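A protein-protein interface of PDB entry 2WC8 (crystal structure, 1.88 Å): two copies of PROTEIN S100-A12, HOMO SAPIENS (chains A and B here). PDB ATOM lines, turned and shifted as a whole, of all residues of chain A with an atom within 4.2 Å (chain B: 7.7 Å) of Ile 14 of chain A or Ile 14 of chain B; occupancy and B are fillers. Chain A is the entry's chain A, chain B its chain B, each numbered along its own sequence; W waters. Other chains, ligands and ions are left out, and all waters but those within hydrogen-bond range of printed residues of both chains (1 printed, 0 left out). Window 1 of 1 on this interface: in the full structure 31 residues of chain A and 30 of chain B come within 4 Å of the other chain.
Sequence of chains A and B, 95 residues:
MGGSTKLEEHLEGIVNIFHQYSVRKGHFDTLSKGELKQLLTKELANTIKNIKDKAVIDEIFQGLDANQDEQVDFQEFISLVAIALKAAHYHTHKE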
ATOM      1  N   LEU A   7     -20.883 -19.102  -2.490  1.00  0.00           N
ATOM      2  CA  LEU A   7     -20.953 -20.460  -1.967  1.00  0.00           C
ATOM      3  C   LEU A   7     -21.427 -21.395  -3.099  1.00  0.00           C
ATOM      4  O   LEU A   7     -20.873 -22.450  -3.325  1.00  0.00           O
ATOM      5  CB  LEU A   7     -21.878 -20.524  -0.747  1.00  0.00           C
ATOM      6  CG  LEU A   7     -22.068 -21.909  -0.136  1.00  0.00           C
ATOM      7  CD1 LEU A   7     -20.702 -22.576   0.275  1.00  0.00           C
ATOM      8  CD2 LEU A   7     -23.030 -21.824   1.028  1.00  0.00           C
ATOM      9  N   HIS A  10     -18.951 -22.467  -5.660  1.00  0.00           N
ATOM     10  CA  HIS A  10     -18.111 -23.567  -5.178  1.00  0.00           C
ATOM     11  C   HIS A  10     -18.814 -24.940  -5.326  1.00  0.00           C
ATOM     12  O   HIS A  10     -18.197 -25.939  -5.732  1.00  0.00           O
ATOM     13  CB  HIS A  10     -17.696 -23.346  -3.771  1.00  0.00           C
ATOM     14  CG  HIS A  10     -16.791 -22.169  -3.607  1.00  0.00           C
ATOM     15  ND1 HIS A  10     -15.643 -22.031  -4.354  1.00  0.00           N
ATOM     16  CD2 HIS A  10     -16.807 -21.138  -2.724  1.00  0.00           C
ATOM     17  CE1 HIS A  10     -15.014 -20.931  -3.969  1.00  0.00           C
ATOM     18  NE2 HIS A  10     -15.705 -20.361  -2.996  1.00  0.00           N
ATOM     19  N   LEU A  11     -20.097 -24.993  -5.001  1.00  0.00           N
ATOM     20  CA  LEU A  11     -20.834 -26.257  -5.112  1.00  0.00           C
ATOM     21  C   LEU A  11     -20.883 -26.716  -6.586  1.00  0.00           C
ATOM     22  O   LEU A  11     -20.677 -27.887  -6.893  1.00  0.00           O
ATOM     23  CB  LEU A  11     -22.204 -26.088  -4.555  1.00  0.00           C
ATOM     24  CG  LEU A  11     -22.298 -25.757  -3.066  1.00  0.00           C
ATOM     25  CD1 LEU A  11     -23.796 -25.574  -2.703  1.00  0.00           C
ATOM     26  CD2 LEU A  11     -21.617 -26.759  -2.182  1.00  0.00           C
ATOM     27  N   GLU A  12     -21.120 -25.755  -7.475  1.00  0.00           N
ATOM     28  CA  GLU A  12     -21.229 -25.999  -8.928  1.00  0.00           C
ATOM     29  C   GLU A  12     -19.909 -26.462  -9.478  1.00  0.00           C
ATOM     30  O   GLU A  12     -19.838 -27.300 -10.401  1.00  0.00           O
ATOM     31  CB  GLU A  12     -21.638 -24.715  -9.652  1.00  0.00           C
ATOM     32  CG  GLU A  12     -23.058 -24.337  -9.461  1.00  0.00           C
ATOM     33  CD  GLU A  12     -23.382 -22.852  -9.742  1.00  0.00           C
ATOM     34  OE1 GLU A  12     -22.560 -22.094 -10.332  1.00  0.00           O
ATOM     35  OE2 GLU A  12     -24.487 -22.456  -9.367  1.00  0.00           O
ATOM     36  N   GLY A  13     -18.837 -25.921  -8.906  1.00  0.00           N
ATOM     37  CA  GLY A  13     -17.515 -26.225  -9.384  1.00  0.00           C
ATOM     38  C   GLY A  13     -17.140 -27.635  -9.012  1.00  0.00           C
ATOM     39  O   GLY A  13     -16.467 -28.320  -9.772  1.00  0.00           O
ATOM     40  N   ILE A  14     -17.540 -28.025  -7.811  1.00  0.00           N
ATOM     41  CA  ILE A  14     -17.330 -29.392  -7.301  1.00  0.00           C
ATOM     42  C   ILE A  14     -18.112 -30.367  -8.189  1.00  0.00           C
ATOM     43  O   ILE A  14     -17.599 -31.388  -8.585  1.00  0.00           O
ATOM     44  CB  ILE A  14     -17.743 -29.524  -5.815  1.00  0.00           C
ATOM     45  CG1 ILE A  14     -16.813 -28.704  -4.921  1.00  0.00           C
ATOM     46  CG2 ILE A  14     -17.748 -30.984  -5.353  1.00  0.00           C
ATOM     47  CD1 ILE A  14     -17.246 -28.572  -3.502  1.00  0.00           C
ATOM     48  N   VAL A  15     -19.359 -30.048  -8.474  1.00  0.00           N
ATOM     49  CA  VAL A  15     -20.141 -30.848  -9.392  1.00  0.00           C
ATOM     50  C   VAL A  15     -19.464 -30.905 -10.778  1.00  0.00           C
ATOM     51  O   VAL A  15     -19.404 -31.985 -11.377  1.00  0.00           O
ATOM     52  CB  VAL A  15     -21.600 -30.337  -9.530  1.00  0.00           C
ATOM     53  CG1 VAL A  15     -22.336 -31.172 -10.614  1.00  0.00           C
ATOM     54  CG2 VAL A  15     -22.385 -30.393  -8.147  1.00  0.00           C
ATOM     55  N   ASN A  16     -18.944 -29.762 -11.262  1.00  0.00           N
ATOM     56  CA  ASN A  16     -18.307 -29.719 -12.544  1.00  0.00           C
ATOM     57  C   ASN A  16     -17.089 -30.646 -12.548  1.00  0.00           C
ATOM     58  O   ASN A  16     -16.870 -31.361 -13.519  1.00  0.00           O
ATOM     59  CB  ASN A  16     -17.929 -28.283 -12.963  1.00  0.00           C
ATOM     60  CG  ASN A  16     -17.274 -28.227 -14.316  1.00  0.00           C
ATOM     61  OD1 ASN A  16     -17.934 -27.957 -15.321  1.00  0.00           O
ATOM     62  ND2 ASN A  16     -15.986 -28.517 -14.361  1.00  0.00           N
ATOM     63  N   ILE A  17     -16.312 -30.666 -11.462  1.00  0.00           N
ATOM     64  CA  ILE A  17     -15.088 -31.468 -11.501  1.00  0.00           C
ATOM     65  C   ILE A  17     -15.434 -32.945 -11.550  1.00  0.00           C
ATOM     66  O   ILE A  17     -14.827 -33.698 -12.276  1.00  0.00           O
ATOM     67  CB  ILE A  17     -14.150 -31.104 -10.358  1.00  0.00           C
ATOM     68  CG1 ILE A  17     -13.597 -29.665 -10.587  1.00  0.00           C
ATOM     69  CG2 ILE A  17     -12.964 -32.123 -10.232  1.00  0.00           C
ATOM     70  CD1 ILE A  17     -13.066 -28.952  -9.309  1.00  0.00           C
ATOM     71  N   PHE A  18     -16.401 -33.337 -10.748  1.00  0.00           N
ATOM     72  CA  PHE A  18     -16.931 -34.681 -10.775  1.00  0.00           C
ATOM     73  C   PHE A  18     -17.281 -35.063 -12.195  1.00  0.00           C
ATOM     74  O   PHE A  18     -16.926 -36.125 -12.674  1.00  0.00           O
ATOM     75  CB  PHE A  18     -18.173 -34.833  -9.873  1.00  0.00           C
ATOM     76  CG  PHE A  18     -18.768 -36.162  -9.947  1.00  0.00           C
ATOM     77  CD1 PHE A  18     -18.214 -37.215  -9.204  1.00  0.00           C
ATOM     78  CD2 PHE A  18     -19.857 -36.412 -10.757  1.00  0.00           C
ATOM     79  CE1 PHE A  18     -18.772 -38.538  -9.270  1.00  0.00           C
ATOM     80  CE2 PHE A  18     -20.411 -37.752 -10.858  1.00  0.00           C
ATOM     81  CZ  PHE A  18     -19.875 -38.787 -10.096  1.00  0.00           C
ATOM     82  N   PHE A  77     -19.440 -39.859  -3.810  1.00  0.00           N
ATOM     83  CA  PHE A  77     -18.447 -38.802  -3.937  1.00  0.00           C
ATOM     84  C   PHE A  77     -18.642 -37.678  -2.927  1.00  0.00           C
ATOM     85  O   PHE A  77     -17.675 -37.162  -2.396  1.00  0.00           O
ATOM     86  CB  PHE A  77     -18.429 -38.255  -5.369  1.00  0.00           C
ATOM     87  CG  PHE A  77     -17.403 -37.212  -5.627  1.00  0.00           C
ATOM     88  CD1 PHE A  77     -17.775 -35.905  -5.874  1.00  0.00           C
ATOM     89  CD2 PHE A  77     -16.039 -37.517  -5.656  1.00  0.00           C
ATOM     90  CE1 PHE A  77     -16.848 -34.938  -6.122  1.00  0.00           C
ATOM     91  CE2 PHE A  77     -15.108 -36.513  -5.900  1.00  0.00           C
ATOM     92  CZ  PHE A  77     -15.521 -35.221  -6.118  1.00  0.00           C
ATOM     93  N   LEU A  85     -13.357 -31.931   3.286  1.00  0.00           N
ATOM     94  CA  LEU A  85     -13.729 -30.642   3.884  1.00  0.00           C
ATOM     95  C   LEU A  85     -13.358 -30.511   5.387  1.00  0.00           C
ATOM     96  O   LEU A  85     -12.835 -29.470   5.819  1.00  0.00           O
ATOM     97  CB  LEU A  85     -15.235 -30.358   3.705  1.00  0.00           C
ATOM     98  CG  LEU A  85     -15.788 -29.620   2.538  1.00  0.00           C
ATOM     99  CD1 LEU A  85     -17.373 -29.610   2.703  1.00  0.00           C
ATOM    100  CD2 LEU A  85     -15.171 -28.172   2.525  1.00  0.00           C
ATOM    101  N   LYS B   6      -8.226 -26.770  -8.437  1.00  0.00           N
ATOM    102  CA  LYS B   6      -9.514 -26.087  -8.450  1.00  0.00           C
ATOM    103  C   LYS B   6     -10.419 -26.711  -7.409  1.00  0.00           C
ATOM    104  O   LYS B   6     -11.100 -26.018  -6.671  1.00  0.00           O
ATOM    105  CB  LYS B   6     -10.167 -26.155  -9.835  1.00  0.00           C
ATOM    106  CG  LYS B   6      -9.694 -25.099 -10.787  1.00  0.00           C
ATOM    107  CD  LYS B   6     -10.421 -25.239 -12.150  1.00  0.00           C
ATOM    108  CE  LYS B   6     -10.308 -23.976 -13.039  1.00  0.00           C
ATOM    109  NZ  LYS B   6      -9.212 -24.162 -14.010  1.00  0.00           N
ATOM    110  N   LEU B   7     -10.407 -28.039  -7.315  1.00  0.00           N
ATOM    111  CA  LEU B   7     -11.231 -28.697  -6.279  1.00  0.00           C
ATOM    112  C   LEU B   7     -10.853 -28.233  -4.873  1.00  0.00           C
ATOM    113  O   LEU B   7     -11.745 -27.966  -4.026  1.00  0.00           O
ATOM    114  CB  LEU B   7     -11.156 -30.231  -6.407  1.00  0.00           C
ATOM    115  CG  LEU B   7     -11.954 -31.002  -5.351  1.00  0.00           C
ATOM    116  CD1 LEU B   7     -13.423 -30.624  -5.413  1.00  0.00           C
ATOM    117  CD2 LEU B   7     -11.656 -32.540  -5.542  1.00  0.00           C
ATOM    118  N   GLU B   8      -9.559 -28.105  -4.612  1.00  0.00           N
ATOM    119  CA  GLU B   8      -9.083 -27.655  -3.318  1.00  0.00           C
ATOM    120  C   GLU B   8      -9.462 -26.210  -3.011  1.00  0.00           C
ATOM    121  O   GLU B   8      -9.860 -25.906  -1.896  1.00  0.00           O
ATOM    122  CB  GLU B   8      -7.613 -27.915  -3.149  1.00  0.00           C
ATOM    123  CG  GLU B   8      -7.333 -29.425  -3.080  1.00  0.00           C
ATOM    124  CD  GLU B   8      -5.890 -29.806  -3.167  1.00  0.00           C
ATOM    125  OE1 GLU B   8      -5.064 -29.161  -3.861  1.00  0.00           O
ATOM    126  OE2 GLU B   8      -5.577 -30.817  -2.533  1.00  0.00           O
ATOM    127  N   GLU B   9      -9.424 -25.363  -4.034  1.00  0.00           N
ATOM    128  CA  GLU B   9      -9.834 -23.953  -3.884  1.00  0.00           C
ATOM    129  C   GLU B   9     -11.314 -23.893  -3.518  1.00  0.00           C
ATOM    130  O   GLU B   9     -11.752 -23.117  -2.654  1.00  0.00           O
ATOM    131  CB  GLU B   9      -9.601 -23.175  -5.179  1.00  0.00           C
ATOM    132  CG  GLU B   9      -8.159 -22.922  -5.614  1.00  0.00           C
ATOM    133  CD  GLU B   9      -8.053 -22.397  -7.079  1.00  0.00           C
ATOM    134  OE1 GLU B   9      -9.064 -22.378  -7.872  1.00  0.00           O
ATOM    135  OE2 GLU B   9      -6.925 -22.056  -7.475  1.00  0.00           O
ATOM    136  N   HIS B  10     -12.118 -24.778  -4.088  1.00  0.00           N
ATOM    137  CA  HIS B  10     -13.545 -24.763  -3.695  1.00  0.00           C
ATOM    138  C   HIS B  10     -13.745 -25.224  -2.256  1.00  0.00           C
ATOM    139  O   HIS B  10     -14.553 -24.637  -1.535  1.00  0.00           O
ATOM    140  CB  HIS B  10     -14.390 -25.632  -4.604  1.00  0.00           C
ATOM    141  CG  HIS B  10     -14.473 -25.142  -6.014  1.00  0.00           C
ATOM    142  ND1 HIS B  10     -14.837 -23.847  -6.337  1.00  0.00           N
ATOM    143  CD2 HIS B  10     -14.329 -25.799  -7.192  1.00  0.00           C
ATOM    144  CE1 HIS B  10     -14.853 -23.718  -7.653  1.00  0.00           C
ATOM    145  NE2 HIS B  10     -14.563 -24.894  -8.197  1.00  0.00           N
ATOM    146  N   LEU B  11     -13.005 -26.229  -1.811  1.00  0.00           N
ATOM    147  CA  LEU B  11     -13.049 -26.642  -0.392  1.00  0.00           C
ATOM    148  C   LEU B  11     -12.653 -25.474   0.550  1.00  0.00           C
ATOM    149  O   LEU B  11     -13.366 -25.161   1.491  1.00  0.00           O
ATOM    150  CB  LEU B  11     -12.130 -27.838  -0.142  1.00  0.00           C
ATOM    151  CG  LEU B  11     -12.368 -29.112  -0.928  1.00  0.00           C
ATOM    152  CD1 LEU B  11     -11.456 -30.215  -0.422  1.00  0.00           C
ATOM    153  CD2 LEU B  11     -13.813 -29.534  -0.860  1.00  0.00           C
ATOM    154  N   GLU B  12     -11.535 -24.832   0.270  1.00  0.00           N
ATOM    155  CA  GLU B  12     -11.116 -23.684   1.022  1.00  0.00           C
ATOM    156  C   GLU B  12     -12.153 -22.544   0.986  1.00  0.00           C
ATOM    157  O   GLU B  12     -12.382 -21.869   1.999  1.00  0.00           O
ATOM    158  CB  GLU B  12      -9.788 -23.174   0.523  1.00  0.00           C
ATOM    159  CG  GLU B  12      -9.194 -22.154   1.489  1.00  0.00           C
ATOM    160  CD  GLU B  12      -7.794 -21.721   1.142  1.00  0.00           C
ATOM    161  OE1 GLU B  12      -7.420 -20.609   1.554  1.00  0.00           O
ATOM    162  OE2 GLU B  12      -7.077 -22.480   0.451  1.00  0.00           O
ATOM    163  N   GLY B  13     -12.741 -22.340  -0.173  1.00  0.00           N
ATOM    164  CA  GLY B  13     -13.806 -21.337  -0.332  1.00  0.00           C
ATOM    165  C   GLY B  13     -15.011 -21.613   0.566  1.00  0.00           C
ATOM    166  O   GLY B  13     -15.489 -20.741   1.229  1.00  0.00           O
ATOM    167  N   ILE B  14     -15.429 -22.870   0.655  1.00  0.00           N
ATOM    168  CA  ILE B  14     -16.498 -23.271   1.568  1.00  0.00           C
ATOM    169  C   ILE B  14     -16.111 -23.008   3.021  1.00  0.00           C
ATOM    170  O   ILE B  14     -16.928 -22.502   3.807  1.00  0.00           O
ATOM    171  CB  ILE B  14     -16.932 -24.747   1.320  1.00  0.00           C
ATOM    172  CG1 ILE B  14     -17.506 -24.896  -0.110  1.00  0.00           C
ATOM    173  CG2 ILE B  14     -17.887 -25.291   2.370  1.00  0.00           C
ATOM    174  CD1 ILE B  14     -17.610 -26.386  -0.616  1.00  0.00           C
ATOM    175  N   VAL B  15     -14.885 -23.366   3.400  1.00  0.00           N
ATOM    176  CA  VAL B  15     -14.420 -23.068   4.739  1.00  0.00           C
ATOM    177  C   VAL B  15     -14.403 -21.566   4.980  1.00  0.00           C
ATOM    178  O   VAL B  15     -14.766 -21.104   6.073  1.00  0.00           O
ATOM    179  CB  VAL B  15     -13.005 -23.582   4.966  1.00  0.00           C
ATOM    180  CG1 VAL B  15     -12.491 -23.081   6.299  1.00  0.00           C
ATOM    181  CG2 VAL B  15     -12.926 -25.146   4.832  1.00  0.00           C
ATOM    182  N   ASN B  16     -13.967 -20.821   3.981  1.00  0.00           N
ATOM    183  CA  ASN B  16     -13.919 -19.386   4.093  1.00  0.00           C
ATOM    184  C   ASN B  16     -15.282 -18.746   4.350  1.00  0.00           C
ATOM    185  O   ASN B  16     -15.394 -17.797   5.130  1.00  0.00           O
ATOM    186  CB  ASN B  16     -13.249 -18.751   2.869  1.00  0.00           C
ATOM    187  CG  ASN B  16     -11.741 -18.907   2.858  1.00  0.00           C
ATOM    188  OD1 ASN B  16     -11.145 -19.188   3.880  1.00  0.00           O
ATOM    189  ND2 ASN B  16     -11.106 -18.706   1.688  1.00  0.00           N
ATOM    190  N   ILE B  17     -16.298 -19.220   3.656  1.00  0.00           N
ATOM    191  CA  ILE B  17     -17.664 -18.681   3.841  1.00  0.00           C
ATOM    192  C   ILE B  17     -18.220 -19.001   5.213  1.00  0.00           C
ATOM    193  O   ILE B  17     -18.838 -18.169   5.830  1.00  0.00           O
ATOM    194  CB  ILE B  17     -18.600 -19.118   2.685  1.00  0.00           C
ATOM    195  CG1 ILE B  17     -18.146 -18.347   1.410  1.00  0.00           C
ATOM    196  CG2 ILE B  17     -20.070 -18.772   3.023  1.00  0.00           C
ATOM    197  CD1 ILE B  17     -18.515 -18.924   0.013  1.00  0.00           C
ATOM    198  N   PHE B  18     -18.006 -20.216   5.699  1.00  0.00           N
ATOM    199  CA  PHE B  18     -18.353 -20.561   7.081  1.00  0.00           C
ATOM    200  C   PHE B  18     -17.676 -19.573   8.041  1.00  0.00           C
ATOM    201  O   PHE B  18     -18.310 -19.046   8.928  1.00  0.00           O
ATOM    202  CB  PHE B  18     -17.908 -21.998   7.390  1.00  0.00           C
ATOM    203  CG  PHE B  18     -18.042 -22.374   8.838  1.00  0.00           C
ATOM    204  CD1 PHE B  18     -19.259 -22.846   9.343  1.00  0.00           C
ATOM    205  CD2 PHE B  18     -16.989 -22.172   9.721  1.00  0.00           C
ATOM    206  CE1 PHE B  18     -19.380 -23.191  10.680  1.00  0.00           C
ATOM    207  CE2 PHE B  18     -17.105 -22.473  11.078  1.00  0.00           C
ATOM    208  CZ  PHE B  18     -18.301 -22.986  11.555  1.00  0.00           C
ATOM    209  N   HIS B  19     -16.394 -19.290   7.822  1.00  0.00           N
ATOM    210  CA  HIS B  19     -15.650 -18.433   8.769  1.00  0.00           C
ATOM    211  C   HIS B  19     -16.096 -16.980   8.703  1.00  0.00           C
ATOM    212  O   HIS B  19     -16.049 -16.255   9.723  1.00  0.00           O
ATOM    213  CB  HIS B  19     -14.130 -18.505   8.555  1.00  0.00           C
ATOM    214  CG  HIS B  19     -13.468 -19.754   9.113  1.00  0.00           C
ATOM    215  ND1 HIS B  19     -12.322 -20.304   8.557  1.00  0.00           N
ATOM    216  CD2 HIS B  19     -13.776 -20.534  10.187  1.00  0.00           C
ATOM    217  CE1 HIS B  19     -11.981 -21.384   9.247  1.00  0.00           C
ATOM    218  NE2 HIS B  19     -12.861 -21.549  10.235  1.00  0.00           N
ATOM    219  N   GLN B  20     -16.522 -16.514   7.524  1.00  0.00           N
ATOM    220  CA  GLN B  20     -16.996 -15.139   7.407  1.00  0.00           C
ATOM    221  C   GLN B  20     -18.254 -14.918   8.234  1.00  0.00           C
ATOM    222  O   GLN B  20     -18.529 -13.802   8.693  1.00  0.00           O
ATOM    223  CB  GLN B  20     -17.205 -14.734   5.938  1.00  0.00           C
ATOM    224  CG  GLN B  20     -18.534 -15.110   5.335  1.00  0.00           C
ATOM    225  CD  GLN B  20     -18.542 -14.863   3.848  1.00  0.00           C
ATOM    226  OE1 GLN B  20     -17.490 -14.570   3.244  1.00  0.00           O
ATOM    227  NE2 GLN B  20     -19.706 -14.996   3.240  1.00  0.00           N
ATOM    228  N   LEU B  39     -27.591 -17.846   6.672  1.00  0.00           N
ATOM    229  CA  LEU B  39     -26.656 -18.349   5.681  1.00  0.00           C
ATOM    230  C   LEU B  39     -27.407 -19.197   4.673  1.00  0.00           C
ATOM    231  O   LEU B  39     -27.273 -18.981   3.443  1.00  0.00           O
ATOM    232  CB  LEU B  39     -25.531 -19.124   6.365  1.00  0.00           C
ATOM    233  CG  LEU B  39     -24.387 -19.685   5.539  1.00  0.00           C
ATOM    234  CD1 LEU B  39     -23.192 -20.017   6.431  1.00  0.00           C
ATOM    235  CD2 LEU B  39     -24.812 -20.929   4.754  1.00  0.00           C
ATOM    236  N   PHE B  74     -18.269 -26.481  12.523  1.00  0.00           N
ATOM    237  CA  PHE B  74     -17.976 -26.780  11.137  1.00  0.00           C
ATOM    238  C   PHE B  74     -18.451 -28.190  10.684  1.00  0.00           C
ATOM    239  O   PHE B  74     -18.922 -28.367   9.538  1.00  0.00           O
ATOM    240  CB  PHE B  74     -16.499 -26.588  10.802  1.00  0.00           C
ATOM    241  CG  PHE B  74     -16.253 -26.605   9.315  1.00  0.00           C
ATOM    242  CD1 PHE B  74     -16.638 -25.510   8.537  1.00  0.00           C
ATOM    243  CD2 PHE B  74     -15.728 -27.701   8.693  1.00  0.00           C
ATOM    244  CE1 PHE B  74     -16.471 -25.524   7.148  1.00  0.00           C
ATOM    245  CE2 PHE B  74     -15.528 -27.710   7.291  1.00  0.00           C
ATOM    246  CZ  PHE B  74     -15.945 -26.637   6.534  1.00  0.00           C
ATOM    247  N   PHE B  77     -22.043 -27.940   9.925  1.00  0.00           N
ATOM    248  CA  PHE B  77     -22.156 -27.240   8.660  1.00  0.00           C
ATOM    249  C   PHE B  77     -21.819 -28.115   7.452  1.00  0.00           C
ATOM    250  O   PHE B  77     -22.472 -28.010   6.415  1.00  0.00           O
ATOM    251  CB  PHE B  77     -21.290 -25.998   8.682  1.00  0.00           C
ATOM    252  CG  PHE B  77     -21.283 -25.214   7.391  1.00  0.00           C
ATOM    253  CD1 PHE B  77     -20.158 -25.215   6.590  1.00  0.00           C
ATOM    254  CD2 PHE B  77     -22.340 -24.340   7.068  1.00  0.00           C
ATOM    255  CE1 PHE B  77     -20.079 -24.424   5.428  1.00  0.00           C
ATOM    256  CE2 PHE B  77     -22.286 -23.563   5.922  1.00  0.00           C
ATOM    257  CZ  PHE B  77     -21.148 -23.574   5.114  1.00  0.00           C
ATOM    258  N   ILE B  78     -20.882 -29.046   7.609  1.00  0.00           N
ATOM    259  CA  ILE B  78     -20.565 -29.978   6.545  1.00  0.00           C
ATOM    260  C   ILE B  78     -21.803 -30.781   6.119  1.00  0.00           C
ATOM    261  O   ILE B  78     -21.979 -31.053   4.920  1.00  0.00           O
ATOM    262  CB  ILE B  78     -19.406 -30.933   6.908  1.00  0.00           C
ATOM    263  CG1 ILE B  78     -18.070 -30.227   6.959  1.00  0.00           C
ATOM    264  CG2 ILE B  78     -19.299 -32.073   5.901  1.00  0.00           C
ATOM    265  CD1 ILE B  78     -16.980 -31.150   7.568  1.00  0.00           C
ATOM    266  N   VAL B  81     -23.640 -28.573   3.785  1.00  0.00           N
ATOM    267  CA  VAL B  81     -22.962 -28.454   2.501  1.00  0.00           C
ATOM    268  C   VAL B  81     -23.260 -29.791   1.687  1.00  0.00           C
ATOM    269  O   VAL B  81     -23.454 -29.732   0.481  1.00  0.00           O
ATOM    270  CB  VAL B  81     -21.457 -28.236   2.671  1.00  0.00           C
ATOM    271  CG1 VAL B  81     -20.742 -28.315   1.293  1.00  0.00           C
ATOM    272  CG2 VAL B  81     -21.175 -26.846   3.404  1.00  0.00           C
ATOM    273  N   LEU B  85     -24.911 -29.905  -1.982  1.00  0.00           N
ATOM    274  CA  LEU B  85     -24.169 -30.421  -3.105  1.00  0.00           C
ATOM    275  C   LEU B  85     -25.027 -31.360  -3.861  1.00  0.00           C
ATOM    276  O   LEU B  85     -24.963 -31.405  -5.086  1.00  0.00           O
ATOM    277  CB  LEU B  85     -22.958 -31.236  -2.643  1.00  0.00           C
ATOM    278  CG  LEU B  85     -21.607 -30.614  -2.588  1.00  0.00           C
ATOM    279  CD1 LEU B  85     -20.674 -31.642  -1.860  1.00  0.00           C
ATOM    280  CD2 LEU B  85     -21.063 -30.270  -3.999  1.00  0.00           C
ATOM    281  N   HIS B  89     -26.158 -30.832  -7.713  1.00  0.00           N
ATOM    282  CA  HIS B  89     -25.983 -31.858  -8.739  1.00  0.00           C
ATOM    283  C   HIS B  89     -27.279 -32.243  -9.425  1.00  0.00           C
ATOM    284  O   HIS B  89     -27.350 -32.295 -10.670  1.00  0.00           O
ATOM    285  CB  HIS B  89     -25.348 -33.099  -8.128  1.00  0.00           C
ATOM    286  CG  HIS B  89     -25.188 -34.221  -9.109  1.00  0.00           C
ATOM    287  ND1 HIS B  89     -25.850 -35.419  -8.976  1.00  0.00           N
ATOM    288  CD2 HIS B  89     -24.478 -34.314 -10.253  1.00  0.00           C
ATOM    289  CE1 HIS B  89     -25.553 -36.202 -10.000  1.00  0.00           C
ATOM    290  NE2 HIS B  89     -24.735 -35.554 -10.795  1.00  0.00           N
HETATM  291  O   HOH W   1     -15.218 -18.234  -1.144  1.00  0.00           O
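A ring nitrogen (ND1) of His 10 of chain B is in hydrogen-bond range of a ring nitrogen (ND1) of His 10 of chain A.
Among the printed residues, merely in contact across the chains: Leu 7 of chain A with Ile 14 of chain B (3.97 Å), Leu 7 of chain A with Ile 17 of chain B (3.5 Å), His 10 of chain A with Gly 13 of chain B (3.4 Å), His 10 of chain A with Ile 14 of chain B (3.98 Å), His 10 of chain A with Ile 17 of chain B (3.9 Å), Leu 11 of chain A with Val 81 of chain B (3.9 Å), Leu 11 of chain A with Leu 85 of chain B (3.8 Å), Gly 13 of chain A with His 10 of chain B (3.4 Å), Ile 14 of chain A with Leu 7 of chain B (3.9 Å), Ile 14 of chain A with His 10 of chain B (3.9 Å), Ile 14 of chain A with Ile 14 of chain B (3.6 Å), Ile 14 of chain A with Leu 85 of chain B (3.7 Å), Val 15 of chain A with His 89 of chain B (3.8 Å), Ile 17 of chain A with Lys 6 of chain B (3.95 Å), Ile 17 of chain A with Leu 7 of chain B (3.4 Å), Leu 85 of chain A with Leu 11 of chain B (3.7 Å), Leu 85 of chain A with Ile 14 of chain B (3.96 Å), Leu 85 of chain A with Phe 74 of chain B (3.5 Å) and Leu 85 of chain A with Val 81 of chain B (3.9 Å).
Of chain B, only His 10 (3.4 Å) comes within 4 Å of Gly 13 of chain A.
Of chain B, only Leu 7, His 10, Ile 14 and Leu 85 come within 4 Å of Ile 14 of chain A.
Printed residues of chain A within 4 Å of Leu 7 of chain B: Ile 14 and Ile 17.
Glu 8 of chain B touches none of the printed residues of chain A.
Glu 12 of chain B touches none of the printed residues of chain A.
Of the printed residues of chain A, Ile 14 of chain B touches Leu 7 (3.97 Å), His 10 (3.98 Å), Ile 14 (3.6 Å) and Leu 85 (3.96 Å).
Printed residues of chain A within 4 Å of Ile 17 of chain B: Leu 7 and His 10.
The nearest residue of chain B that does not touch Ile 14 of chain A is Leu 11 of chain B (4.4 Å).
Of the 12 printed residues of chain A, 8 touch a printed residue of chain B.
Hydrophobic or aromatic side chains of chain A that line the printed part of chain B: Leu 7, His 10, Leu 11, Ile 14, Val 15, Ile 17 and Leu 85.
Hydrophobic or aromatic side chains of chain B within 4 Å of the printed part of chain A: Leu 7, His 10, Leu 11, Ile 14, Ile 17, Phe 74, Val 81, Leu 85 and His 89.
Among the printed residues, 20 pairs touch across the chains.
Among the printed residues, no Asp or Glu carboxylate lies within 4 Å of a Lys or Arg side-chain nitrogen of the other chain.
Leu 7 of chain A touches Ile 14 of chain B, and with the chains exchanged Ile 14 of chain A touches Leu 7 of chain B.
His 10 of chain A touches its own counterpart, His 10 of chain B.
His 10 of chain A touches Ile 17 of chain B, but with the chains exchanged Ile 17 of chain A does not touch His 10 of chain B (4.002 Å).
Leu 11 of chain A touches Leu 85 of chain B, and with the chains exchanged Leu 85 of chain A touches Leu 11 of chain B.
Positions printed for both chains: 7, 10, 11, 12, 13, 14, 15, 16, 17, 18, 77 and 85.
Of the 20 pairs that touch across the chains among the printed residues, 14 have their exchanged pair printed and touching as well.
Water W1 bridges a ring nitrogen (NE2) of His 10 of chain A (2.9 Å) and the backbone carbonyl oxygen (O) of Gly 13 of chain B (3.5 Å).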
